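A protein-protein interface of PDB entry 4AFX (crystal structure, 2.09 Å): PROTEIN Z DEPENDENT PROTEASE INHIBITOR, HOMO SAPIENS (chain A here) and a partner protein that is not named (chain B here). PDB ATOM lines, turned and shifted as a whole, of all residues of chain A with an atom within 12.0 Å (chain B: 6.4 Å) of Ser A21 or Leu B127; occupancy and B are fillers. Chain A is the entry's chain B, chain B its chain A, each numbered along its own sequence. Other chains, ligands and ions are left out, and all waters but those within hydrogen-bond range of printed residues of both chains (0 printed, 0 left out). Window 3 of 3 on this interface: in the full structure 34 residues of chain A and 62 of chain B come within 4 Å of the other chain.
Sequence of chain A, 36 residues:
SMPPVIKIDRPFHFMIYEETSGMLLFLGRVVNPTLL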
ATOM      1  N   ILE A  16      13.800  16.550 -21.954  1.00  0.00           N
ATOM      2  CA  ILE A  16      12.899  17.679 -21.910  1.00  0.00           C
ATOM      3  C   ILE A  16      13.688  18.887 -22.422  1.00  0.00           C
ATOM      4  O   ILE A  16      14.742  19.246 -21.832  1.00  0.00           O
ATOM      5  CB  ILE A  16      12.405  17.950 -20.486  1.00  0.00           C
ATOM      6  CG1 ILE A  16      11.670  16.711 -19.948  1.00  0.00           C
ATOM      7  CG2 ILE A  16      11.519  19.236 -20.456  1.00  0.00           C
ATOM      8  CD1 ILE A  16      10.964  16.881 -18.579  1.00  0.00           C
ATOM      9  N   TYR A  17      13.190  19.469 -23.528  1.00  0.00           N
ATOM     10  CA  TYR A  17      13.830  20.538 -24.287  1.00  0.00           C
ATOM     11  C   TYR A  17      12.973  21.778 -24.285  1.00  0.00           C
ATOM     12  O   TYR A  17      11.767  21.676 -24.428  1.00  0.00           O
ATOM     13  CB  TYR A  17      13.855  20.160 -25.769  1.00  0.00           C
ATOM     14  CG  TYR A  17      15.010  19.367 -26.168  1.00  0.00           C
ATOM     15  CD1 TYR A  17      16.235  19.970 -26.388  1.00  0.00           C
ATOM     16  CD2 TYR A  17      14.900  17.981 -26.322  1.00  0.00           C
ATOM     17  CE1 TYR A  17      17.358  19.215 -26.768  1.00  0.00           C
ATOM     18  CE2 TYR A  17      16.009  17.217 -26.679  1.00  0.00           C
ATOM     19  CZ  TYR A  17      17.233  17.842 -26.904  1.00  0.00           C
ATOM     20  OH  TYR A  17      18.327  17.092 -27.265  1.00  0.00           O
ATOM     21  N   GLU A  18      13.588  22.948 -24.216  1.00  0.00           N
ATOM     22  CA  GLU A  18      12.879  24.156 -24.526  1.00  0.00           C
ATOM     23  C   GLU A  18      13.155  24.421 -26.016  1.00  0.00           C
ATOM     24  O   GLU A  18      14.307  24.507 -26.425  1.00  0.00           O
ATOM     25  CB  GLU A  18      13.371  25.304 -23.639  1.00  0.00           C
ATOM     26  CG  GLU A  18      12.468  26.542 -23.697  1.00  0.00           C
ATOM     27  CD  GLU A  18      12.680  27.340 -24.955  1.00  0.00           C
ATOM     28  OE1 GLU A  18      13.858  27.635 -25.255  1.00  0.00           O
ATOM     29  OE2 GLU A  18      11.682  27.653 -25.648  1.00  0.00           O
ATOM     30  N   GLU A  19      12.103  24.568 -26.809  1.00  0.00           N
ATOM     31  CA  GLU A  19      12.212  24.482 -28.273  1.00  0.00           C
ATOM     32  C   GLU A  19      12.762  25.715 -28.997  1.00  0.00           C
ATOM     33  O   GLU A  19      13.431  25.557 -30.026  1.00  0.00           O
ATOM     34  CB  GLU A  19      10.871  24.046 -28.866  1.00  0.00           C
ATOM     35  CG  GLU A  19      10.577  22.592 -28.490  1.00  0.00           C
ATOM     36  CD  GLU A  19       9.321  22.029 -29.139  1.00  0.00           C
ATOM     37  OE1 GLU A  19       8.194  22.252 -28.596  1.00  0.00           O
ATOM     38  OE2 GLU A  19       9.479  21.354 -30.190  1.00  0.00           O
ATOM     39  N   THR A  20      12.532  26.896 -28.441  1.00  0.00           N
ATOM     40  CA  THR A  20      13.081  28.170 -28.966  1.00  0.00           C
ATOM     41  C   THR A  20      14.609  28.202 -28.806  1.00  0.00           C
ATOM     42  O   THR A  20      15.350  28.347 -29.783  1.00  0.00           O
ATOM     43  CB  THR A  20      12.427  29.396 -28.245  1.00  0.00           C
ATOM     44  OG1 THR A  20      11.014  29.350 -28.454  1.00  0.00           O
ATOM     45  CG2 THR A  20      12.924  30.730 -28.759  1.00  0.00           C
ATOM     46  N   SER A  21      15.087  28.028 -27.581  1.00  0.00           N
ATOM     47  CA  SER A  21      16.534  27.959 -27.342  1.00  0.00           C
ATOM     48  C   SER A  21      17.151  26.630 -27.785  1.00  0.00           C
ATOM     49  O   SER A  21      18.319  26.599 -28.150  1.00  0.00           O
ATOM     50  CB  SER A  21      16.860  28.191 -25.866  1.00  0.00           C
ATOM     51  OG  SER A  21      16.374  27.152 -25.061  1.00  0.00           O
ATOM     52  N   GLY A  22      16.376  25.544 -27.778  1.00  0.00           N
ATOM     53  CA  GLY A  22      16.960  24.223 -27.961  1.00  0.00           C
ATOM     54  C   GLY A  22      17.700  23.722 -26.702  1.00  0.00           C
ATOM     55  O   GLY A  22      18.433  22.740 -26.766  1.00  0.00           O
ATOM     56  N   MET A  23      17.487  24.384 -25.565  1.00  0.00           N
ATOM     57  CA  MET A  23      18.139  24.017 -24.321  1.00  0.00           C
ATOM     58  C   MET A  23      17.561  22.727 -23.698  1.00  0.00           C
ATOM     59  O   MET A  23      16.343  22.609 -23.480  1.00  0.00           O
ATOM     60  CB  MET A  23      18.017  25.187 -23.327  1.00  0.00           C
ATOM     61  CG  MET A  23      18.894  25.061 -22.089  1.00  0.00           C
ATOM     62  SD  MET A  23      20.675  24.846 -22.498  1.00  0.00           S
ATOM     63  CE  MET A  23      21.077  26.419 -23.190  1.00  0.00           C
ATOM     64  N   LEU A  24      18.451  21.787 -23.377  1.00  0.00           N
ATOM     65  CA  LEU A  24      18.085  20.506 -22.804  1.00  0.00           C
ATOM     66  C   LEU A  24      18.015  20.670 -21.296  1.00  0.00           C
ATOM     67  O   LEU A  24      19.041  20.832 -20.621  1.00  0.00           O
ATOM     68  CB  LEU A  24      19.110  19.432 -23.218  1.00  0.00           C
ATOM     69  CG  LEU A  24      18.827  18.007 -22.793  1.00  0.00           C
ATOM     70  CD1 LEU A  24      17.494  17.482 -23.291  1.00  0.00           C
ATOM     71  CD2 LEU A  24      19.981  17.090 -23.258  1.00  0.00           C
ATOM     72  N   LEU A  25      16.784  20.647 -20.784  1.00  0.00           N
ATOM     73  CA  LEU A  25      16.480  20.961 -19.398  1.00  0.00           C
ATOM     74  C   LEU A  25      16.677  19.758 -18.491  1.00  0.00           C
ATOM     75  O   LEU A  25      17.113  19.897 -17.353  1.00  0.00           O
ATOM     76  CB  LEU A  25      15.039  21.494 -19.249  1.00  0.00           C
ATOM     77  CG  LEU A  25      14.665  22.801 -19.965  1.00  0.00           C
ATOM     78  CD1 LEU A  25      13.147  23.215 -19.798  1.00  0.00           C
ATOM     79  CD2 LEU A  25      15.553  24.003 -19.584  1.00  0.00           C
ATOM     80  N   PHE A  26      16.294  18.585 -18.989  1.00  0.00           N
ATOM     81  CA  PHE A  26      16.329  17.334 -18.215  1.00  0.00           C
ATOM     82  C   PHE A  26      16.548  16.174 -19.184  1.00  0.00           C
ATOM     83  O   PHE A  26      16.049  16.184 -20.295  1.00  0.00           O
ATOM     84  CB  PHE A  26      15.008  17.119 -17.441  1.00  0.00           C
ATOM     85  CG  PHE A  26      14.756  18.144 -16.382  1.00  0.00           C
ATOM     86  CD1 PHE A  26      15.236  17.963 -15.102  1.00  0.00           C
ATOM     87  CD2 PHE A  26      14.041  19.295 -16.666  1.00  0.00           C
ATOM     88  CE1 PHE A  26      15.028  18.932 -14.120  1.00  0.00           C
ATOM     89  CE2 PHE A  26      13.852  20.284 -15.709  1.00  0.00           C
ATOM     90  CZ  PHE A  26      14.324  20.102 -14.434  1.00  0.00           C
ATOM     91  N   ARG B  51      23.643  32.037 -28.591  1.00  0.00           N
ATOM     92  CA  ARG B  51      22.737  31.323 -27.723  1.00  0.00           C
ATOM     93  C   ARG B  51      22.409  29.933 -28.300  1.00  0.00           C
ATOM     94  O   ARG B  51      22.296  28.971 -27.573  1.00  0.00           O
ATOM     95  CB  ARG B  51      21.453  32.121 -27.570  1.00  0.00           C
ATOM     96  CG  ARG B  51      20.633  31.721 -26.374  1.00  0.00           C
ATOM     97  CD  ARG B  51      19.339  32.534 -26.287  1.00  0.00           C
ATOM     98  NE  ARG B  51      19.522  33.884 -25.746  1.00  0.00           N
ATOM     99  CZ  ARG B  51      18.513  34.712 -25.466  1.00  0.00           C
ATOM    100  NH1 ARG B  51      17.261  34.313 -25.666  1.00  0.00           N
ATOM    101  NH2 ARG B  51      18.743  35.935 -24.996  1.00  0.00           N
ATOM    102  N   GLN B  52      22.262  29.847 -29.607  1.00  0.00           N
ATOM    103  CA  GLN B  52      22.068  28.569 -30.294  1.00  0.00           C
ATOM    104  C   GLN B  52      23.255  27.652 -30.051  1.00  0.00           C
ATOM    105  O   GLN B  52      23.087  26.487 -29.768  1.00  0.00           O
ATOM    106  CB  GLN B  52      21.824  28.773 -31.807  1.00  0.00           C
ATOM    107  CG  GLN B  52      20.440  29.373 -32.098  1.00  0.00           C
ATOM    108  CD  GLN B  52      20.223  29.918 -33.535  1.00  0.00           C
ATOM    109  OE1 GLN B  52      21.095  29.807 -34.433  1.00  0.00           O
ATOM    110  NE2 GLN B  52      19.044  30.530 -33.744  1.00  0.00           N
ATOM    111  N   LEU B  54      25.344  27.773 -27.469  1.00  0.00           N
ATOM    112  CA  LEU B  54      25.383  27.404 -26.078  1.00  0.00           C
ATOM    113  C   LEU B  54      24.462  26.220 -25.804  1.00  0.00           C
ATOM    114  O   LEU B  54      24.844  25.255 -25.148  1.00  0.00           O
ATOM    115  CB  LEU B  54      24.971  28.592 -25.207  1.00  0.00           C
ATOM    116  CG  LEU B  54      24.918  28.371 -23.710  1.00  0.00           C
ATOM    117  CD1 LEU B  54      26.307  27.936 -23.162  1.00  0.00           C
ATOM    118  CD2 LEU B  54      24.443  29.603 -23.012  1.00  0.00           C
ATOM    119  N   ALA B  55      23.239  26.337 -26.281  1.00  0.00           N
ATOM    120  CA  ALA B  55      22.274  25.271 -26.223  1.00  0.00           C
ATOM    121  C   ALA B  55      22.799  23.991 -26.885  1.00  0.00           C
ATOM    122  O   ALA B  55      22.847  22.967 -26.238  1.00  0.00           O
ATOM    123  CB  ALA B  55      20.946  25.747 -26.874  1.00  0.00           C
ATOM    124  N   LYS B  56      23.230  24.042 -28.147  1.00  0.00           N
ATOM    125  CA  LYS B  56      23.771  22.830 -28.784  1.00  0.00           C
ATOM    126  C   LYS B  56      24.896  22.151 -27.983  1.00  0.00           C
ATOM    127  O   LYS B  56      24.893  20.918 -27.780  1.00  0.00           O
ATOM    128  CB  LYS B  56      24.261  23.126 -30.189  1.00  0.00           C
ATOM    129  CG  LYS B  56      24.755  21.878 -30.953  1.00  0.00           C
ATOM    130  CD  LYS B  56      25.142  22.191 -32.421  1.00  0.00           C
ATOM    131  CE  LYS B  56      26.453  22.989 -32.498  1.00  0.00           C
ATOM    132  NZ  LYS B  56      26.545  23.872 -33.709  1.00  0.00           N
ATOM    133  N   PHE B  82      21.297  21.629 -18.484  1.00  0.00           N
ATOM    134  CA  PHE B  82      21.202  23.065 -18.343  1.00  0.00           C
ATOM    135  C   PHE B  82      21.654  23.497 -16.952  1.00  0.00           C
ATOM    136  O   PHE B  82      22.472  24.421 -16.798  1.00  0.00           O
ATOM    137  CB  PHE B  82      19.765  23.511 -18.628  1.00  0.00           C
ATOM    138  CG  PHE B  82      19.516  24.982 -18.387  1.00  0.00           C
ATOM    139  CD1 PHE B  82      20.195  25.934 -19.089  1.00  0.00           C
ATOM    140  CD2 PHE B  82      18.586  25.397 -17.440  1.00  0.00           C
ATOM    141  CE1 PHE B  82      19.964  27.318 -18.859  1.00  0.00           C
ATOM    142  CE2 PHE B  82      18.346  26.754 -17.231  1.00  0.00           C
ATOM    143  CZ  PHE B  82      19.053  27.715 -17.948  1.00  0.00           C
ATOM    144  N   SER B 122      26.675  36.136 -19.419  1.00  0.00           N
ATOM    145  CA  SER B 122      25.687  37.064 -19.990  1.00  0.00           C
ATOM    146  C   SER B 122      24.664  36.291 -20.856  1.00  0.00           C
ATOM    147  O   SER B 122      23.520  36.654 -20.929  1.00  0.00           O
ATOM    148  CB  SER B 122      26.355  38.190 -20.799  1.00  0.00           C
ATOM    149  OG  SER B 122      26.577  37.725 -22.125  1.00  0.00           O
ATOM    150  N   LEU B 123      25.095  35.193 -21.481  1.00  0.00           N
ATOM    151  CA  LEU B 123      24.194  34.355 -22.267  1.00  0.00           C
ATOM    152  C   LEU B 123      23.191  33.637 -21.393  1.00  0.00           C
ATOM    153  O   LEU B 123      22.022  33.522 -21.760  1.00  0.00           O
ATOM    154  CB  LEU B 123      24.984  33.319 -23.069  1.00  0.00           C
ATOM    155  CG  LEU B 123      25.764  33.919 -24.235  1.00  0.00           C
ATOM    156  CD1 LEU B 123      26.372  32.816 -25.095  1.00  0.00           C
ATOM    157  CD2 LEU B 123      24.849  34.818 -25.078  1.00  0.00           C
ATOM    158  N   PHE B 124      23.626  33.106 -20.250  1.00  0.00           N
ATOM    159  CA  PHE B 124      22.655  32.510 -19.356  1.00  0.00           C
ATOM    160  C   PHE B 124      21.715  33.574 -18.780  1.00  0.00           C
ATOM    161  O   PHE B 124      20.539  33.313 -18.582  1.00  0.00           O
ATOM    162  CB  PHE B 124      23.305  31.718 -18.227  1.00  0.00           C
ATOM    163  CG  PHE B 124      23.897  30.423 -18.652  1.00  0.00           C
ATOM    164  CD1 PHE B 124      23.084  29.306 -18.877  1.00  0.00           C
ATOM    165  CD2 PHE B 124      25.272  30.300 -18.837  1.00  0.00           C
ATOM    166  CE1 PHE B 124      23.656  28.078 -19.266  1.00  0.00           C
ATOM    167  CE2 PHE B 124      25.819  29.106 -19.230  1.00  0.00           C
ATOM    168  CZ  PHE B 124      25.034  27.980 -19.420  1.00  0.00           C
ATOM    169  N   LYS B 125      22.222  34.777 -18.503  1.00  0.00           N
ATOM    170  CA  LYS B 125      21.348  35.830 -18.029  1.00  0.00           C
ATOM    171  C   LYS B 125      20.272  36.144 -19.074  1.00  0.00           C
ATOM    172  O   LYS B 125      19.078  36.213 -18.743  1.00  0.00           O
ATOM    173  CB  LYS B 125      22.152  37.092 -17.699  1.00  0.00           C
ATOM    174  CG  LYS B 125      21.303  38.365 -17.502  1.00  0.00           C
ATOM    175  CD  LYS B 125      22.205  39.576 -17.298  1.00  0.00           C
ATOM    176  CE  LYS B 125      21.424  40.854 -16.966  1.00  0.00           C
ATOM    177  NZ  LYS B 125      20.667  40.677 -15.710  1.00  0.00           N
ATOM    178  N   GLY B 126      20.690  36.365 -20.323  1.00  0.00           N
ATOM    179  CA  GLY B 126      19.752  36.696 -21.397  1.00  0.00           C
ATOM    180  C   GLY B 126      18.748  35.567 -21.570  1.00  0.00           C
ATOM    181  O   GLY B 126      17.543  35.793 -21.748  1.00  0.00           O
ATOM    182  N   LEU B 127      19.245  34.337 -21.490  1.00  0.00           N
ATOM    183  CA  LEU B 127      18.392  33.191 -21.630  1.00  0.00           C
ATOM    184  C   LEU B 127      17.412  33.082 -20.450  1.00  0.00           C
ATOM    185  O   LEU B 127      16.227  32.816 -20.653  1.00  0.00           O
ATOM    186  CB  LEU B 127      19.219  31.924 -21.816  1.00  0.00           C
ATOM    187  CG  LEU B 127      18.406  30.807 -22.439  1.00  0.00           C
ATOM    188  CD1 LEU B 127      18.195  31.095 -23.909  1.00  0.00           C
ATOM    189  CD2 LEU B 127      19.018  29.420 -22.241  1.00  0.00           C
ATOM    190  N   ARG B 128      17.878  33.316 -19.237  1.00  0.00           N
ATOM    191  CA  ARG B 128      16.983  33.359 -18.084  1.00  0.00           C
ATOM    192  C   ARG B 128      15.874  34.420 -18.227  1.00  0.00           C
ATOM    193  O   ARG B 128      14.728  34.137 -17.897  1.00  0.00           O
ATOM    194  CB  ARG B 128      17.793  33.594 -16.809  1.00  0.00           C
ATOM    195  CG  ARG B 128      16.983  33.808 -15.517  1.00  0.00           C
ATOM    196  CD  ARG B 128      17.908  33.717 -14.299  1.00  0.00           C
ATOM    197  NE  ARG B 128      18.955  34.732 -14.370  1.00  0.00           N
ATOM    198  CZ  ARG B 128      18.782  36.005 -14.027  1.00  0.00           C
ATOM    199  NH1 ARG B 128      17.609  36.410 -13.565  1.00  0.00           N
ATOM    200  NH2 ARG B 128      19.777  36.881 -14.150  1.00  0.00           N
ATOM    201  N   GLU B 129      16.187  35.623 -18.721  1.00  0.00           N
ATOM    202  CA  GLU B 129      15.170  36.707 -18.812  1.00  0.00           C
ATOM    203  C   GLU B 129      14.098  36.410 -19.854  1.00  0.00           C
ATOM    204  O   GLU B 129      12.936  36.746 -19.661  1.00  0.00           O
ATOM    205  CB  GLU B 129      15.812  38.076 -19.108  1.00  0.00           C
ATOM    206  CG  GLU B 129      16.765  38.571 -17.999  1.00  0.00           C
ATOM    207  CD  GLU B 129      17.716  39.694 -18.435  1.00  0.00           C
ATOM    208  OE1 GLU B 129      17.890  39.955 -19.642  1.00  0.00           O
ATOM    209  OE2 GLU B 129      18.317  40.310 -17.539  1.00  0.00           O
ATOM    210  N   THR B 130      14.484  35.779 -20.959  1.00  0.00           N
ATOM    211  CA  THR B 130      13.495  35.353 -21.958  1.00  0.00           C
ATOM    212  C   THR B 130      12.661  34.155 -21.453  1.00  0.00           C
ATOM    213  O   THR B 130      11.444  34.184 -21.481  1.00  0.00           O
ATOM    214  CB  THR B 130      14.133  35.033 -23.321  1.00  0.00           C
ATOM    215  OG1 THR B 130      14.812  33.787 -23.231  1.00  0.00           O
ATOM    216  CG2 THR B 130      15.099  36.127 -23.772  1.00  0.00           C
ATOM    217  N   LEU B 131      13.300  33.107 -20.962  1.00  0.00           N
ATOM    218  CA  LEU B 131      12.529  31.979 -20.428  1.00  0.00           C
ATOM    219  C   LEU B 131      11.586  32.411 -19.276  1.00  0.00           C
ATOM    220  O   LEU B 131      10.487  31.878 -19.150  1.00  0.00           O
ATOM    221  CB  LEU B 131      13.445  30.847 -19.981  1.00  0.00           C
ATOM    222  CG  LEU B 131      14.351  30.250 -21.073  1.00  0.00           C
ATOM    223  CD1 LEU B 131      15.121  29.081 -20.510  1.00  0.00           C
ATOM    224  CD2 LEU B 131      13.587  29.868 -22.371  1.00  0.00           C
ATOM    225  N   SER B 132      11.998  33.391 -18.463  1.00  0.00           N
ATOM    226  CA  SER B 132      11.139  33.904 -17.374  1.00  0.00           C
ATOM    227  C   SER B 132       9.899  34.654 -17.865  1.00  0.00           C
ATOM    228  O   SER B 132       8.911  34.737 -17.130  1.00  0.00           O
ATOM    229  CB  SER B 132      11.920  34.811 -16.410  1.00  0.00           C
ATOM    230  OG  SER B 132      12.557  34.041 -15.401  1.00  0.00           O
ATOM    231  N   GLN B 141      14.249  29.536 -12.205  1.00  0.00           N
ATOM    232  CA  GLN B 141      15.574  29.207 -11.791  1.00  0.00           C
ATOM    233  C   GLN B 141      16.099  30.247 -10.816  1.00  0.00           C
ATOM    234  O   GLN B 141      15.595  31.380 -10.711  1.00  0.00           O
ATOM    235  CB  GLN B 141      16.503  29.078 -13.008  1.00  0.00           C
ATOM    236  CG  GLN B 141      16.494  30.287 -13.920  1.00  0.00           C
ATOM    237  CD  GLN B 141      17.228  30.066 -15.226  1.00  0.00           C
ATOM    238  OE1 GLN B 141      18.439  30.007 -15.236  1.00  0.00           O
ATOM    239  NE2 GLN B 141      16.492  29.997 -16.347  1.00  0.00           N
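The backbone NH of Phe B82 is in hydrogen-bond range of the backbone carbonyl oxygen of Leu A24, 3.2 Å away.
O of Leu B127 lies within hydrogen-bond range of OG1 of Thr B130, 3.1 Å away. The backbone carbonyl oxygen (O) of Ile A16 sits at hydrogen-bond distance from the backbone NH (N) of Leu A25. The backbone NH (N) of Thr A20 lies within hydrogen-bond range of the side-chain carboxylate (OE2) of Glu A18 (3.0 Å). OG of Ser A21 is in hydrogen-bond range of OE1 of Glu A18 (2.6 Å). The backbone NH (N) of Glu A18 is in hydrogen-bond range of the backbone carbonyl oxygen (O) of Met A23 (2.9 Å). OG of Ser A21 is in hydrogen-bond range of N of Met A23 (3.0 Å).
Leu B131 touches Glu A18. Ala B55 touches Ser A21. Leu B127 touches Ser A21. Gly A22 touches Ala B55. Ala B55 touches Met A23. Met A23 touches Phe B82. Met A23 touches Leu B127 (CE to CD2, 3.8 Å). Phe B82 touches Leu A25.
Ser A21 touches just these residues of chain B: Ala B55 (3.0 Å) and Leu B127 (3.7 Å). Printed residues of chain A within 4 Å of Leu B127: Ser A21 (3.7 Å) and Met A23 (3.8 Å). No residue of chain A comes within 4 Å of Gln B52. No residue of chain A comes within 4 Å of Leu B54. No residue of chain A comes within 4 Å of Leu B123. No residue of chain A comes within 4 Å of Phe B124. Gly B126 touches none of the printed residues of chain A. No residue of chain A comes within 4 Å of Arg B128. No residue of chain A comes within 4 Å of Glu B129. Printed residues of chain B within 4 Å of Leu A25: Phe B82. Printed residues of chain B within 4 Å of Gly A22: Ala B55 (3.8 Å). Of the printed residues of chain A, Phe B82 touches Met A23 (3.4 Å), Leu A24 (3.2 Å) and Leu A25 (3.97 Å). Printed residues of chain B within 4 Å of Leu A24: Phe B82 (3.2 Å). Of the printed residues of chain B, Met A23 touches Ala B55 (3.5 Å), Phe B82 (3.4 Å) and Leu B127 (3.8 Å). The nearest residue of chain B that does not touch Ser A21 is Arg B51 (4.7 Å). The nearest residue of chain A that does not touch Leu B127 is Glu A18 (5.7 Å). The nearest printed residue of chain B that does not touch Met A23 is Leu B54 (4.3 Å).
Of the 18 printed residues of chain B, 4 touch a printed residue of chain A. Printed residues of chain B that touch a printed residue of chain A: Ala B55, Phe B82, Leu B127 and Leu B131. Along chain B the printed residues that touch a printed residue of chain A span positions 55 to 131. Of the 11 printed residues of chain A, 6 touch a printed residue of chain B. Hydrophobic or aromatic side chains of chain A within 4 Å of the printed part of chain B: Met A23 and Leu A25.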
